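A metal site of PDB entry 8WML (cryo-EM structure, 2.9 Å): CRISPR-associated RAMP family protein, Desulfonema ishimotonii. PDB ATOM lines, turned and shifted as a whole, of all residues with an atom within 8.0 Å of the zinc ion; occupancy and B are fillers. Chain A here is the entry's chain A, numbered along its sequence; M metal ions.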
ATOM      1  N   ARG A 684      -4.289  -4.640  -3.033  1.00  0.00           N
ATOM      2  CA  ARG A 684      -4.390  -3.281  -2.502  1.00  0.00           C
ATOM      3  C   ARG A 684      -4.357  -2.250  -3.630  1.00  0.00           C
ATOM      4  O   ARG A 684      -5.145  -1.301  -3.630  1.00  0.00           O
ATOM      5  CB  ARG A 684      -3.254  -3.034  -1.513  1.00  0.00           C
ATOM      6  CG  ARG A 684      -3.259  -1.650  -0.888  1.00  0.00           C
ATOM      7  CD  ARG A 684      -2.275  -1.578   0.261  1.00  0.00           C
ATOM      8  NE  ARG A 684      -2.384  -0.318   0.986  1.00  0.00           N
ATOM      9  CZ  ARG A 684      -1.826   0.831   0.593  1.00  0.00           C
ATOM     10  NH1 ARG A 684      -1.117   0.916  -0.510  1.00  0.00           N
ATOM     11  NH2 ARG A 684      -2.003   1.918   1.350  1.00  0.00           N
ATOM     12  N   CYS A 706      -6.209   9.700   9.429  1.00  0.00           N
ATOM     13  CA  CYS A 706      -6.997   9.300   8.281  1.00  0.00           C
ATOM     14  C   CYS A 706      -7.966   8.189   8.663  1.00  0.00           C
ATOM     15  O   CYS A 706      -7.692   7.409   9.572  1.00  0.00           O
ATOM     16  CB  CYS A 706      -6.096   8.847   7.135  1.00  0.00           C
ATOM     17  SG  CYS A 706      -6.958   8.230   5.675  1.00  0.00           S
ATOM     18  N   GLU A 707      -9.120   8.166   7.989  1.00  0.00           N
ATOM     19  CA  GLU A 707     -10.179   7.154   8.264  1.00  0.00           C
ATOM     20  C   GLU A 707     -10.747   6.676   6.930  1.00  0.00           C
ATOM     21  O   GLU A 707     -11.918   6.251   6.915  1.00  0.00           O
ATOM     22  CB  GLU A 707     -11.333   7.819   9.020  1.00  0.00           C
ATOM     23  CG  GLU A 707     -12.448   6.860   9.421  1.00  0.00           C
ATOM     24  CD  GLU A 707     -13.466   6.493   8.348  1.00  0.00           C
ATOM     25  OE1 GLU A 707     -13.643   7.290   7.398  1.00  0.00           O
ATOM     26  OE2 GLU A 707     -14.079   5.410   8.478  1.00  0.00           O
ATOM     27  N   CYS A 708      -9.962   6.769   5.854  1.00  0.00           N
ATOM     28  CA  CYS A 708     -10.408   6.367   4.533  1.00  0.00           C
ATOM     29  C   CYS A 708     -10.611   4.850   4.448  1.00  0.00           C
ATOM     30  O   CYS A 708     -10.195   4.090   5.338  1.00  0.00           O
ATOM     31  CB  CYS A 708      -9.394   6.812   3.472  1.00  0.00           C
ATOM     32  SG  CYS A 708      -7.781   6.012   3.584  1.00  0.00           S
ATOM     33  N   LEU A 709     -11.262   4.410   3.371  1.00  0.00           N
ATOM     34  CA  LEU A 709     -11.615   3.001   3.209  1.00  0.00           C
ATOM     35  C   LEU A 709     -10.368   2.125   3.170  1.00  0.00           C
ATOM     36  O   LEU A 709     -10.338   1.055   3.786  1.00  0.00           O
ATOM     37  CB  LEU A 709     -12.443   2.828   1.941  1.00  0.00           C
ATOM     38  CG  LEU A 709     -13.111   1.477   1.682  1.00  0.00           C
ATOM     39  CD1 LEU A 709     -14.515   1.684   1.135  1.00  0.00           C
ATOM     40  CD2 LEU A 709     -12.292   0.633   0.730  1.00  0.00           C
ATOM     41  N   LEU A 710      -9.342   2.574   2.450  1.00  0.00           N
ATOM     42  CA  LEU A 710      -8.117   1.792   2.347  1.00  0.00           C
ATOM     43  C   LEU A 710      -7.460   1.631   3.708  1.00  0.00           C
ATOM     44  O   LEU A 710      -7.028   0.533   4.076  1.00  0.00           O
ATOM     45  CB  LEU A 710      -7.152   2.477   1.365  1.00  0.00           C
ATOM     46  CG  LEU A 710      -6.154   1.566   0.633  1.00  0.00           C
ATOM     47  CD1 LEU A 710      -6.852   0.756  -0.443  1.00  0.00           C
ATOM     48  CD2 LEU A 710      -5.043   2.400   0.033  1.00  0.00           C
ATOM     49  N   CYS A 711      -7.400   2.706   4.486  1.00  0.00           N
ATOM     50  CA  CYS A 711      -6.817   2.619   5.822  1.00  0.00           C
ATOM     51  C   CYS A 711      -7.632   1.678   6.704  1.00  0.00           C
ATOM     52  O   CYS A 711      -7.064   0.843   7.409  1.00  0.00           O
ATOM     53  CB  CYS A 711      -6.736   4.003   6.455  1.00  0.00           C
ATOM     54  SG  CYS A 711      -5.329   4.995   5.884  1.00  0.00           S
ATOM     55  N   GLN A 712      -8.960   1.792   6.659  1.00  0.00           N
ATOM     56  CA  GLN A 712      -9.790   0.962   7.528  1.00  0.00           C
ATOM     57  C   GLN A 712      -9.638  -0.518   7.193  1.00  0.00           C
ATOM     58  O   GLN A 712      -9.600  -1.359   8.093  1.00  0.00           O
ATOM     59  CB  GLN A 712     -11.262   1.375   7.426  1.00  0.00           C
ATOM     60  CG  GLN A 712     -11.661   2.705   8.068  1.00  0.00           C
ATOM     61  CD  GLN A 712     -11.099   2.924   9.462  1.00  0.00           C
ATOM     62  OE1 GLN A 712     -11.636   2.416  10.450  1.00  0.00           O
ATOM     63  NE2 GLN A 712     -10.005   3.667   9.554  1.00  0.00           N
ATOM     64  N   GLY A 715      -5.339  -1.487   7.116  1.00  0.00           N
ATOM     65  CA  GLY A 715      -4.501  -0.993   8.190  1.00  0.00           C
ATOM     66  C   GLY A 715      -3.558   0.103   7.704  1.00  0.00           C
ATOM     67  O   GLY A 715      -3.497   0.443   6.532  1.00  0.00           O
ATOM     68  N   SER A 716      -2.809   0.647   8.654  1.00  0.00           N
ATOM     69  CA  SER A 716      -1.841   1.708   8.375  1.00  0.00           C
ATOM     70  C   SER A 716      -0.801   1.699   9.494  1.00  0.00           C
ATOM     71  O   SER A 716      -0.743   0.768  10.300  1.00  0.00           O
ATOM     72  CB  SER A 716      -2.549   3.063   8.250  1.00  0.00           C
ATOM     73  OG  SER A 716      -3.059   3.499   9.490  1.00  0.00           O
ATOM     74  N   GLU A 719      -2.740   1.865  12.908  1.00  0.00           N
ATOM     75  CA  GLU A 719      -3.781   0.891  13.231  1.00  0.00           C
ATOM     76  C   GLU A 719      -3.519  -0.397  12.474  1.00  0.00           C
ATOM     77  O   GLU A 719      -2.972  -0.384  11.373  1.00  0.00           O
ATOM     78  CB  GLU A 719      -5.174   1.445  12.896  1.00  0.00           C
ATOM     79  CG  GLU A 719      -5.492   1.520  11.405  1.00  0.00           C
ATOM     80  CD  GLU A 719      -6.227   2.792  11.031  1.00  0.00           C
ATOM     81  OE1 GLU A 719      -7.400   2.966  11.459  1.00  0.00           O
ATOM     82  OE2 GLU A 719      -5.649   3.626  10.311  1.00  0.00           O
HETATM   83 ZN    ZN M   1      -5.765   6.721   4.423  1.00  0.00          ZN
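Along chain A the residues within 4 Å of the zinc ion span positions 706 to 711.
SG of Cys 706 is bound to the zinc ion.
SG of Cys 708 is bound to the zinc ion.
The side-chain sulfur (SG) of Cys 711 is bound to the zinc ion (2.3 Å).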
